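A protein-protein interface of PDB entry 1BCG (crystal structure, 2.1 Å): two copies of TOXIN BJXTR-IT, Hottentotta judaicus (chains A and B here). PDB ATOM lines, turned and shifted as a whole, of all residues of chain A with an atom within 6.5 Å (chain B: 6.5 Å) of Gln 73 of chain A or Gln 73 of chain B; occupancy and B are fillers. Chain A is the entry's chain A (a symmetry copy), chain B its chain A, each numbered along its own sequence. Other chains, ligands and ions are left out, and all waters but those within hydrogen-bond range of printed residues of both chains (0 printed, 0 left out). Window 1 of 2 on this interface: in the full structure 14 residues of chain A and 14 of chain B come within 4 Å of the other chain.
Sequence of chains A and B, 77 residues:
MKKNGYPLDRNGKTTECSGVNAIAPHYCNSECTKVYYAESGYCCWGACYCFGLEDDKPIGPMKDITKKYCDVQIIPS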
ATOM      1  N   PRO A  25     -35.591 -10.775  11.221  1.00  0.00           N
ATOM      2  CA  PRO A  25     -35.351 -11.741  10.139  1.00  0.00           C
ATOM      3  C   PRO A  25     -36.424 -12.812   9.952  1.00  0.00           C
ATOM      4  O   PRO A  25     -36.527 -13.414   8.888  1.00  0.00           O
ATOM      5  CB  PRO A  25     -34.021 -12.389  10.546  1.00  0.00           C
ATOM      6  CG  PRO A  25     -33.422 -11.405  11.544  1.00  0.00           C
ATOM      7  CD  PRO A  25     -34.649 -11.035  12.321  1.00  0.00           C
ATOM      8  N   ASN A  29     -36.936 -15.203   6.816  1.00  0.00           N
ATOM      9  CA  ASN A  29     -36.305 -16.496   7.056  1.00  0.00           C
ATOM     10  C   ASN A  29     -37.311 -17.609   6.786  1.00  0.00           C
ATOM     11  O   ASN A  29     -36.959 -18.653   6.238  1.00  0.00           O
ATOM     12  CB  ASN A  29     -35.759 -16.574   8.486  1.00  0.00           C
ATOM     13  CG  ASN A  29     -35.024 -17.876   8.760  1.00  0.00           C
ATOM     14  OD1 ASN A  29     -35.620 -18.876   9.167  1.00  0.00           O
ATOM     15  ND2 ASN A  29     -33.723 -17.876   8.508  1.00  0.00           N
ATOM     16  N   GLU A  39     -31.468 -22.174   3.068  1.00  0.00           N
ATOM     17  CA  GLU A  39     -30.989 -22.447   4.426  1.00  0.00           C
ATOM     18  C   GLU A  39     -31.457 -21.405   5.442  1.00  0.00           C
ATOM     19  O   GLU A  39     -31.694 -21.725   6.600  1.00  0.00           O
ATOM     20  CB  GLU A  39     -29.458 -22.513   4.446  1.00  0.00           C
ATOM     21  CG  GLU A  39     -28.859 -23.542   3.504  1.00  0.00           C
ATOM     22  CD  GLU A  39     -27.338 -23.555   3.548  1.00  0.00           C
ATOM     23  OE1 GLU A  39     -26.725 -22.481   3.374  1.00  0.00           O
ATOM     24  OE2 GLU A  39     -26.755 -24.639   3.748  1.00  0.00           O
ATOM     25  N   SER A  40     -31.578 -20.156   5.000  1.00  0.00           N
ATOM     26  CA  SER A  40     -32.020 -19.074   5.870  1.00  0.00           C
ATOM     27  C   SER A  40     -32.226 -17.805   5.049  1.00  0.00           C
ATOM     28  O   SER A  40     -32.061 -17.808   3.828  1.00  0.00           O
ATOM     29  CB  SER A  40     -30.985 -18.806   6.962  1.00  0.00           C
ATOM     30  OG  SER A  40     -29.778 -18.299   6.410  1.00  0.00           O
ATOM     31  N   GLY A  41     -32.584 -16.721   5.724  1.00  0.00           N
ATOM     32  CA  GLY A  41     -32.792 -15.462   5.032  1.00  0.00           C
ATOM     33  C   GLY A  41     -33.157 -14.328   5.966  1.00  0.00           C
ATOM     34  O   GLY A  41     -33.423 -14.548   7.152  1.00  0.00           O
ATOM     35  N   TYR A  42     -33.148 -13.108   5.435  1.00  0.00           N
ATOM     36  CA  TYR A  42     -33.505 -11.927   6.210  1.00  0.00           C
ATOM     37  C   TYR A  42     -33.906 -10.833   5.229  1.00  0.00           C
ATOM     38  O   TYR A  42     -33.855 -11.041   4.013  1.00  0.00           O
ATOM     39  CB  TYR A  42     -32.329 -11.485   7.097  1.00  0.00           C
ATOM     40  CG  TYR A  42     -31.169 -10.797   6.393  1.00  0.00           C
ATOM     41  CD1 TYR A  42     -30.204 -11.530   5.706  1.00  0.00           C
ATOM     42  CD2 TYR A  42     -31.016  -9.411   6.460  1.00  0.00           C
ATOM     43  CE1 TYR A  42     -29.106 -10.895   5.104  1.00  0.00           C
ATOM     44  CE2 TYR A  42     -29.930  -8.769   5.867  1.00  0.00           C
ATOM     45  CZ  TYR A  42     -28.979  -9.513   5.196  1.00  0.00           C
ATOM     46  OH  TYR A  42     -27.895  -8.876   4.638  1.00  0.00           O
ATOM     47  N   TYR A  49     -33.838 -11.652   1.220  1.00  0.00           N
ATOM     48  CA  TYR A  49     -32.596 -12.153   0.640  1.00  0.00           C
ATOM     49  C   TYR A  49     -32.368 -13.515   1.302  1.00  0.00           C
ATOM     50  O   TYR A  49     -32.404 -13.614   2.533  1.00  0.00           O
ATOM     51  CB  TYR A  49     -31.455 -11.210   1.005  1.00  0.00           C
ATOM     52  CG  TYR A  49     -30.154 -11.481   0.288  1.00  0.00           C
ATOM     53  CD1 TYR A  49     -29.942 -11.014  -1.008  1.00  0.00           C
ATOM     54  CD2 TYR A  49     -29.134 -12.204   0.905  1.00  0.00           C
ATOM     55  CE1 TYR A  49     -28.746 -11.254  -1.676  1.00  0.00           C
ATOM     56  CE2 TYR A  49     -27.931 -12.451   0.244  1.00  0.00           C
ATOM     57  CZ  TYR A  49     -27.747 -11.971  -1.048  1.00  0.00           C
ATOM     58  OH  TYR A  49     -26.570 -12.219  -1.716  1.00  0.00           O
ATOM     59  N   PHE A  51     -30.107 -17.330   1.722  1.00  0.00           N
ATOM     60  CA  PHE A  51     -28.796 -17.972   1.644  1.00  0.00           C
ATOM     61  C   PHE A  51     -29.004 -19.457   1.389  1.00  0.00           C
ATOM     62  O   PHE A  51     -29.956 -20.049   1.890  1.00  0.00           O
ATOM     63  CB  PHE A  51     -28.007 -17.831   2.955  1.00  0.00           C
ATOM     64  CG  PHE A  51     -27.669 -16.417   3.323  1.00  0.00           C
ATOM     65  CD1 PHE A  51     -28.592 -15.611   3.978  1.00  0.00           C
ATOM     66  CD2 PHE A  51     -26.424 -15.886   3.001  1.00  0.00           C
ATOM     67  CE1 PHE A  51     -28.277 -14.297   4.310  1.00  0.00           C
ATOM     68  CE2 PHE A  51     -26.101 -14.574   3.327  1.00  0.00           C
ATOM     69  CZ  PHE A  51     -27.027 -13.780   3.981  1.00  0.00           C
ATOM     70  N   CYS A  70     -25.535  -7.443   1.151  1.00  0.00           N
ATOM     71  CA  CYS A  70     -26.494  -8.431   1.642  1.00  0.00           C
ATOM     72  C   CYS A  70     -25.925  -9.755   2.166  1.00  0.00           C
ATOM     73  O   CYS A  70     -26.515 -10.362   3.054  1.00  0.00           O
ATOM     74  CB  CYS A  70     -27.560  -8.712   0.574  1.00  0.00           C
ATOM     75  SG  CYS A  70     -28.641  -7.301   0.154  1.00  0.00           S
ATOM     76  N   ASP A  71     -24.794 -10.214   1.638  1.00  0.00           N
ATOM     77  CA  ASP A  71     -24.226 -11.478   2.116  1.00  0.00           C
ATOM     78  C   ASP A  71     -23.686 -11.419   3.544  1.00  0.00           C
ATOM     79  O   ASP A  71     -22.532 -11.064   3.756  1.00  0.00           O
ATOM     80  CB  ASP A  71     -23.112 -11.961   1.184  1.00  0.00           C
ATOM     81  CG  ASP A  71     -23.636 -12.425  -0.157  1.00  0.00           C
ATOM     82  OD1 ASP A  71     -24.559 -13.261  -0.176  1.00  0.00           O
ATOM     83  OD2 ASP A  71     -23.117 -11.968  -1.193  1.00  0.00           O
ATOM     84  N   VAL A  72     -24.519 -11.783   4.518  1.00  0.00           N
ATOM     85  CA  VAL A  72     -24.126 -11.773   5.931  1.00  0.00           C
ATOM     86  C   VAL A  72     -25.008 -12.734   6.747  1.00  0.00           C
ATOM     87  O   VAL A  72     -26.226 -12.743   6.571  1.00  0.00           O
ATOM     88  CB  VAL A  72     -24.267 -10.345   6.553  1.00  0.00           C
ATOM     89  CG1 VAL A  72     -23.767 -10.352   7.990  1.00  0.00           C
ATOM     90  CG2 VAL A  72     -23.493  -9.324   5.737  1.00  0.00           C
ATOM     91  N   GLN A  73     -24.383 -13.534   7.622  1.00  0.00           N
ATOM     92  CA  GLN A  73     -25.069 -14.499   8.505  1.00  0.00           C
ATOM     93  C   GLN A  73     -25.115 -15.982   8.121  1.00  0.00           C
ATOM     94  O   GLN A  73     -24.862 -16.836   8.969  1.00  0.00           O
ATOM     95  CB  GLN A  73     -26.502 -14.041   8.808  1.00  0.00           C
ATOM     96  CG  GLN A  73     -26.690 -13.419  10.183  1.00  0.00           C
ATOM     97  CD  GLN A  73     -26.533 -14.431  11.309  1.00  0.00           C
ATOM     98  OE1 GLN A  73     -26.601 -14.081  12.486  1.00  0.00           O
ATOM     99  NE2 GLN A  73     -26.332 -15.692  10.949  1.00  0.00           N
ATOM    100  N   ILE A  74     -25.429 -16.282   6.861  1.00  0.00           N
ATOM    101  CA  ILE A  74     -25.549 -17.657   6.347  1.00  0.00           C
ATOM    102  C   ILE A  74     -26.194 -18.672   7.293  1.00  0.00           C
ATOM    103  O   ILE A  74     -27.444 -18.725   7.331  1.00  0.00           O
ATOM    104  CB  ILE A  74     -24.187 -18.266   5.868  1.00  0.00           C
ATOM    105  CG1 ILE A  74     -23.143 -18.282   6.995  1.00  0.00           C
ATOM    106  CG2 ILE A  74     -23.697 -17.515   4.644  1.00  0.00           C
ATOM    107  CD1 ILE A  74     -22.488 -16.948   7.305  1.00  0.00           C
ATOM    108  N   PRO B  25     -27.870  -6.139  10.105  1.00  0.00           N
ATOM    109  CA  PRO B  25     -27.041  -7.009  10.951  1.00  0.00           C
ATOM    110  C   PRO B  25     -25.564  -6.633  11.049  1.00  0.00           C
ATOM    111  O   PRO B  25     -24.877  -7.033  11.984  1.00  0.00           O
ATOM    112  CB  PRO B  25     -27.194  -8.383  10.284  1.00  0.00           C
ATOM    113  CG  PRO B  25     -28.449  -8.239   9.431  1.00  0.00           C
ATOM    114  CD  PRO B  25     -28.240  -6.862   8.879  1.00  0.00           C
ATOM    115  N   ASN B  29     -22.907  -7.927  13.711  1.00  0.00           N
ATOM    116  CA  ASN B  29     -22.139  -9.037  13.161  1.00  0.00           C
ATOM    117  C   ASN B  29     -20.650  -8.754  13.324  1.00  0.00           C
ATOM    118  O   ASN B  29     -19.869  -9.658  13.622  1.00  0.00           O
ATOM    119  CB  ASN B  29     -22.503  -9.272  11.691  1.00  0.00           C
ATOM    120  CG  ASN B  29     -21.783 -10.471  11.096  1.00  0.00           C
ATOM    121  OD1 ASN B  29     -20.671 -10.358  10.574  1.00  0.00           O
ATOM    122  ND2 ASN B  29     -22.406 -11.636  11.197  1.00  0.00           N
ATOM    123  N   GLU B  39     -19.241 -16.651  15.439  1.00  0.00           N
ATOM    124  CA  GLU B  39     -19.397 -16.934  14.010  1.00  0.00           C
ATOM    125  C   GLU B  39     -20.170 -15.843  13.269  1.00  0.00           C
ATOM    126  O   GLU B  39     -19.904 -15.573  12.104  1.00  0.00           O
ATOM    127  CB  GLU B  39     -20.109 -18.276  13.809  1.00  0.00           C
ATOM    128  CG  GLU B  39     -19.420 -19.460  14.466  1.00  0.00           C
ATOM    129  CD  GLU B  39     -20.174 -20.763  14.252  1.00  0.00           C
ATOM    130  OE1 GLU B  39     -21.384 -20.812  14.559  1.00  0.00           O
ATOM    131  OE2 GLU B  39     -19.557 -21.742  13.787  1.00  0.00           O
ATOM    132  N   SER B  40     -21.133 -15.230  13.950  1.00  0.00           N
ATOM    133  CA  SER B  40     -21.937 -14.169  13.356  1.00  0.00           C
ATOM    134  C   SER B  40     -22.833 -13.545  14.420  1.00  0.00           C
ATOM    135  O   SER B  40     -22.779 -13.920  15.592  1.00  0.00           O
ATOM    136  CB  SER B  40     -22.806 -14.723  12.226  1.00  0.00           C
ATOM    137  OG  SER B  40     -23.784 -15.623  12.728  1.00  0.00           O
ATOM    138  N   GLY B  41     -23.660 -12.593  14.006  1.00  0.00           N
ATOM    139  CA  GLY B  41     -24.560 -11.947  14.944  1.00  0.00           C
ATOM    140  C   GLY B  41     -25.456 -10.917  14.288  1.00  0.00           C
ATOM    141  O   GLY B  41     -25.264 -10.567  13.119  1.00  0.00           O
ATOM    142  N   TYR B  42     -26.449 -10.444  15.037  1.00  0.00           N
ATOM    143  CA  TYR B  42     -27.370  -9.430  14.544  1.00  0.00           C
ATOM    144  C   TYR B  42     -28.001  -8.751  15.754  1.00  0.00           C
ATOM    145  O   TYR B  42     -27.714  -9.124  16.895  1.00  0.00           O
ATOM    146  CB  TYR B  42     -28.436 -10.060  13.633  1.00  0.00           C
ATOM    147  CG  TYR B  42     -29.529 -10.863  14.322  1.00  0.00           C
ATOM    148  CD1 TYR B  42     -29.307 -12.170  14.747  1.00  0.00           C
ATOM    149  CD2 TYR B  42     -30.803 -10.322  14.504  1.00  0.00           C
ATOM    150  CE1 TYR B  42     -30.335 -12.926  15.334  1.00  0.00           C
ATOM    151  CE2 TYR B  42     -31.833 -11.062  15.084  1.00  0.00           C
ATOM    152  CZ  TYR B  42     -31.595 -12.361  15.492  1.00  0.00           C
ATOM    153  OH  TYR B  42     -32.623 -13.094  16.038  1.00  0.00           O
ATOM    154  N   TYR B  49     -26.888  -9.960  19.502  1.00  0.00           N
ATOM    155  CA  TYR B  49     -27.015 -11.375  19.835  1.00  0.00           C
ATOM    156  C   TYR B  49     -26.033 -12.094  18.906  1.00  0.00           C
ATOM    157  O   TYR B  49     -26.065 -11.876  17.690  1.00  0.00           O
ATOM    158  CB  TYR B  49     -28.437 -11.837  19.532  1.00  0.00           C
ATOM    159  CG  TYR B  49     -28.775 -13.219  20.036  1.00  0.00           C
ATOM    160  CD1 TYR B  49     -29.139 -13.425  21.366  1.00  0.00           C
ATOM    161  CD2 TYR B  49     -28.733 -14.322  19.185  1.00  0.00           C
ATOM    162  CE1 TYR B  49     -29.458 -14.693  21.840  1.00  0.00           C
ATOM    163  CE2 TYR B  49     -29.049 -15.599  19.650  1.00  0.00           C
ATOM    164  CZ  TYR B  49     -29.411 -15.773  20.981  1.00  0.00           C
ATOM    165  OH  TYR B  49     -29.713 -17.029  21.455  1.00  0.00           O
ATOM    166  N   PHE B  51     -23.934 -15.771  17.521  1.00  0.00           N
ATOM    167  CA  PHE B  51     -24.030 -17.217  17.331  1.00  0.00           C
ATOM    168  C   PHE B  51     -22.622 -17.793  17.321  1.00  0.00           C
ATOM    169  O   PHE B  51     -21.693 -17.162  16.825  1.00  0.00           O
ATOM    170  CB  PHE B  51     -24.690 -17.578  15.992  1.00  0.00           C
ATOM    171  CG  PHE B  51     -26.114 -17.125  15.864  1.00  0.00           C
ATOM    172  CD1 PHE B  51     -26.417 -15.825  15.480  1.00  0.00           C
ATOM    173  CD2 PHE B  51     -27.158 -18.004  16.141  1.00  0.00           C
ATOM    174  CE1 PHE B  51     -27.740 -15.407  15.371  1.00  0.00           C
ATOM    175  CE2 PHE B  51     -28.482 -17.594  16.037  1.00  0.00           C
ATOM    176  CZ  PHE B  51     -28.773 -16.297  15.651  1.00  0.00           C
ATOM    177  N   CYS B  70     -34.649 -15.101  19.451  1.00  0.00           N
ATOM    178  CA  CYS B  70     -33.375 -14.654  18.891  1.00  0.00           C
ATOM    179  C   CYS B  70     -32.580 -15.673  18.065  1.00  0.00           C
ATOM    180  O   CYS B  70     -31.862 -15.287  17.148  1.00  0.00           O
ATOM    181  CB  CYS B  70     -32.482 -14.075  19.997  1.00  0.00           C
ATOM    182  SG  CYS B  70     -33.107 -12.556  20.794  1.00  0.00           S
ATOM    183  N   ASP B  71     -32.693 -16.963  18.368  1.00  0.00           N
ATOM    184  CA  ASP B  71     -31.944 -17.962  17.599  1.00  0.00           C
ATOM    185  C   ASP B  71     -32.423 -18.127  16.157  1.00  0.00           C
ATOM    186  O   ASP B  71     -33.329 -18.909  15.890  1.00  0.00           O
ATOM    187  CB  ASP B  71     -31.984 -19.325  18.293  1.00  0.00           C
ATOM    188  CG  ASP B  71     -31.175 -19.351  19.571  1.00  0.00           C
ATOM    189  OD1 ASP B  71     -29.994 -18.960  19.533  1.00  0.00           O
ATOM    190  OD2 ASP B  71     -31.713 -19.776  20.611  1.00  0.00           O
ATOM    191  N   VAL B  72     -31.802 -17.399  15.230  1.00  0.00           N
ATOM    192  CA  VAL B  72     -32.162 -17.464  13.810  1.00  0.00           C
ATOM    193  C   VAL B  72     -30.987 -17.008  12.929  1.00  0.00           C
ATOM    194  O   VAL B  72     -30.350 -16.001  13.233  1.00  0.00           O
ATOM    195  CB  VAL B  72     -33.387 -16.545  13.490  1.00  0.00           C
ATOM    196  CG1 VAL B  72     -33.791 -16.705  12.031  1.00  0.00           C
ATOM    197  CG2 VAL B  72     -34.561 -16.879  14.394  1.00  0.00           C
ATOM    198  N   GLN B  73     -30.709 -17.759  11.854  1.00  0.00           N
ATOM    199  CA  GLN B  73     -29.635 -17.463  10.886  1.00  0.00           C
ATOM    200  C   GLN B  73     -28.295 -18.201  10.983  1.00  0.00           C
ATOM    201  O   GLN B  73     -27.783 -18.664   9.966  1.00  0.00           O
ATOM    202  CB  GLN B  73     -29.344 -15.956  10.835  1.00  0.00           C
ATOM    203  CG  GLN B  73     -29.937 -15.238   9.633  1.00  0.00           C
ATOM    204  CD  GLN B  73     -29.271 -15.640   8.325  1.00  0.00           C
ATOM    205  OE1 GLN B  73     -29.667 -15.192   7.251  1.00  0.00           O
ATOM    206  NE2 GLN B  73     -28.248 -16.481   8.415  1.00  0.00           N
ATOM    207  N   ILE B  74     -27.741 -18.313  12.191  1.00  0.00           N
ATOM    208  CA  ILE B  74     -26.443 -18.962  12.444  1.00  0.00           C
ATOM    209  C   ILE B  74     -25.354 -18.712  11.400  1.00  0.00           C
ATOM    210  O   ILE B  74     -24.688 -17.656  11.490  1.00  0.00           O
ATOM    211  CB  ILE B  74     -26.549 -20.513  12.645  1.00  0.00           C
ATOM    212  CG1 ILE B  74     -27.182 -21.203  11.428  1.00  0.00           C
ATOM    213  CG2 ILE B  74     -27.304 -20.809  13.928  1.00  0.00           C
ATOM    214  CD1 ILE B  74     -28.690 -21.072  11.306  1.00  0.00           C
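The side-chain hydroxyl of Ser 40 of chain B lies within hydrogen-bond range of the side-chain amide nitrogen of Gln 73 of chain A, at 3.1 Å.
The side-chain hydroxyl (OG) of Ser 40 of chain A lies within hydrogen-bond range of the side-chain amide nitrogen (NE2) of Gln 73 of chain B (3.1 Å).
The side-chain amide nitrogen (NE2) of Gln 73 of chain B lies close to the side-chain amide nitrogen (NE2) of Gln 73 of chain A (3.3 Å).
O of Ile 74 of chain A sits at hydrogen-bond distance from NE2 of Gln 73 of chain B (2.6 Å).
NE2 of Gln 73 of chain A sits at hydrogen-bond distance from O of Ile 74 of chain B, at 2.6 Å.
Of the printed residues of chain B, Gln 73 of chain A touches Ser 40, Gly 41, Phe 51, Gln 73 and Ile 74.
Printed residues of chain A within 4 Å of Gln 73 of chain B: Ser 40 (3.1 Å), Gly 41 (3.6 Å), Phe 51 (3.4 Å), Gln 73 (3.0 Å) and Ile 74 (2.6 Å).
Of the printed residues of chain A, Pro 25 of chain B touches Tyr 42.
Printed residues of chain A within 4 Å of Phe 51 of chain B: Gln 73 (3.4 Å).
Of the printed residues of chain B, Tyr 42 of chain A touches Pro 25.
Printed residues of chain B within 4 Å of Gly 41 of chain A: Gln 73.
Of the printed residues of chain A, Tyr 42 of chain B touches Pro 25 (3.9 Å).
Tyr 49 of chain A touches none of the printed residues of chain B.
Asp 71 of chain B touches none of the printed residues of chain A.
The nearest printed residue of chain A that does not touch Gln 73 of chain B is Tyr 42 of chain A (4.01 Å).
The nearest printed residue of chain B that does not touch Phe 51 of chain A is Pro 25 of chain B (7.9 Å).
Asn 29 of chain A touches Val 72 of chain B, and with the chains exchanged Val 72 of chain A touches Asn 29 of chain B.
Ser 40 of chain A touches Gln 73 of chain B, and with the chains exchanged Gln 73 of chain A touches Ser 40 of chain B.
Gly 41 of chain A touches Gln 73 of chain B, and with the chains exchanged Gln 73 of chain A touches Gly 41 of chain B.
Gln 73 of chain B touches its own counterpart, Gln 73 of chain A.
13 positions are printed for both chains.
Among the printed residues, pairs that only touch across the chains: Pro 25 of chain A with Tyr 42 of chain B (3.9 Å), Asn 29 of chain A with Val 72 of chain B (3.7 Å), Gly 41 of chain A with Gln 73 of chain B (3.6 Å), Tyr 42 of chain A with Pro 25 of chain B (3.9 Å), Phe 51 of chain A with Gln 73 of chain B (3.4 Å), Val 72 of chain A with Asn 29 of chain B (3.7 Å), Gln 73 of chain A with Gly 41 of chain B (3.6 Å) and Gln 73 of chain A with Phe 51 of chain B (3.4 Å).
Of the 13 printed residues of chain B, 9 touch a printed residue of chain A.
Hydrophobic or aromatic side chains of chain B within 4 Å of the printed part of chain A: Pro 25, Tyr 42, Phe 51 and Val 72.
Of the 13 printed residues of chain A, 9 touch a printed residue of chain B.
Among the printed residues, no Asp or Glu carboxylate lies within 4 Å of a Lys or Arg side-chain nitrogen of the other chain.
The backbone NH (N) of Glu 39 of chain B is in hydrogen-bond range of the backbone carbonyl oxygen (O) of Phe 51 of chain B, 2.9 Å away.
The backbone NH (N) of Phe 51 of chain B lies within hydrogen-bond range of the backbone carbonyl oxygen (O) of Ser 40 of chain B.
The backbone NH (N) of Tyr 49 of chain B is in hydrogen-bond range of the backbone carbonyl oxygen (O) of Tyr 42 of chain B (2.9 Å).
The backbone carbonyl oxygen (O) of Ser 40 of chain A sits at hydrogen-bond distance from the backbone NH (N) of Phe 51 of chain A, 2.9 Å away.
The backbone carbonyl oxygen (O) of Tyr 42 of chain A sits at hydrogen-bond distance from the backbone NH (N) of Tyr 49 of chain A (2.9 Å).
The side-chain hydroxyl (OH) of Tyr 42 of chain A is in hydrogen-bond range of the backbone carbonyl oxygen (O) of Cys 70 of chain A, at 2.6 Å.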
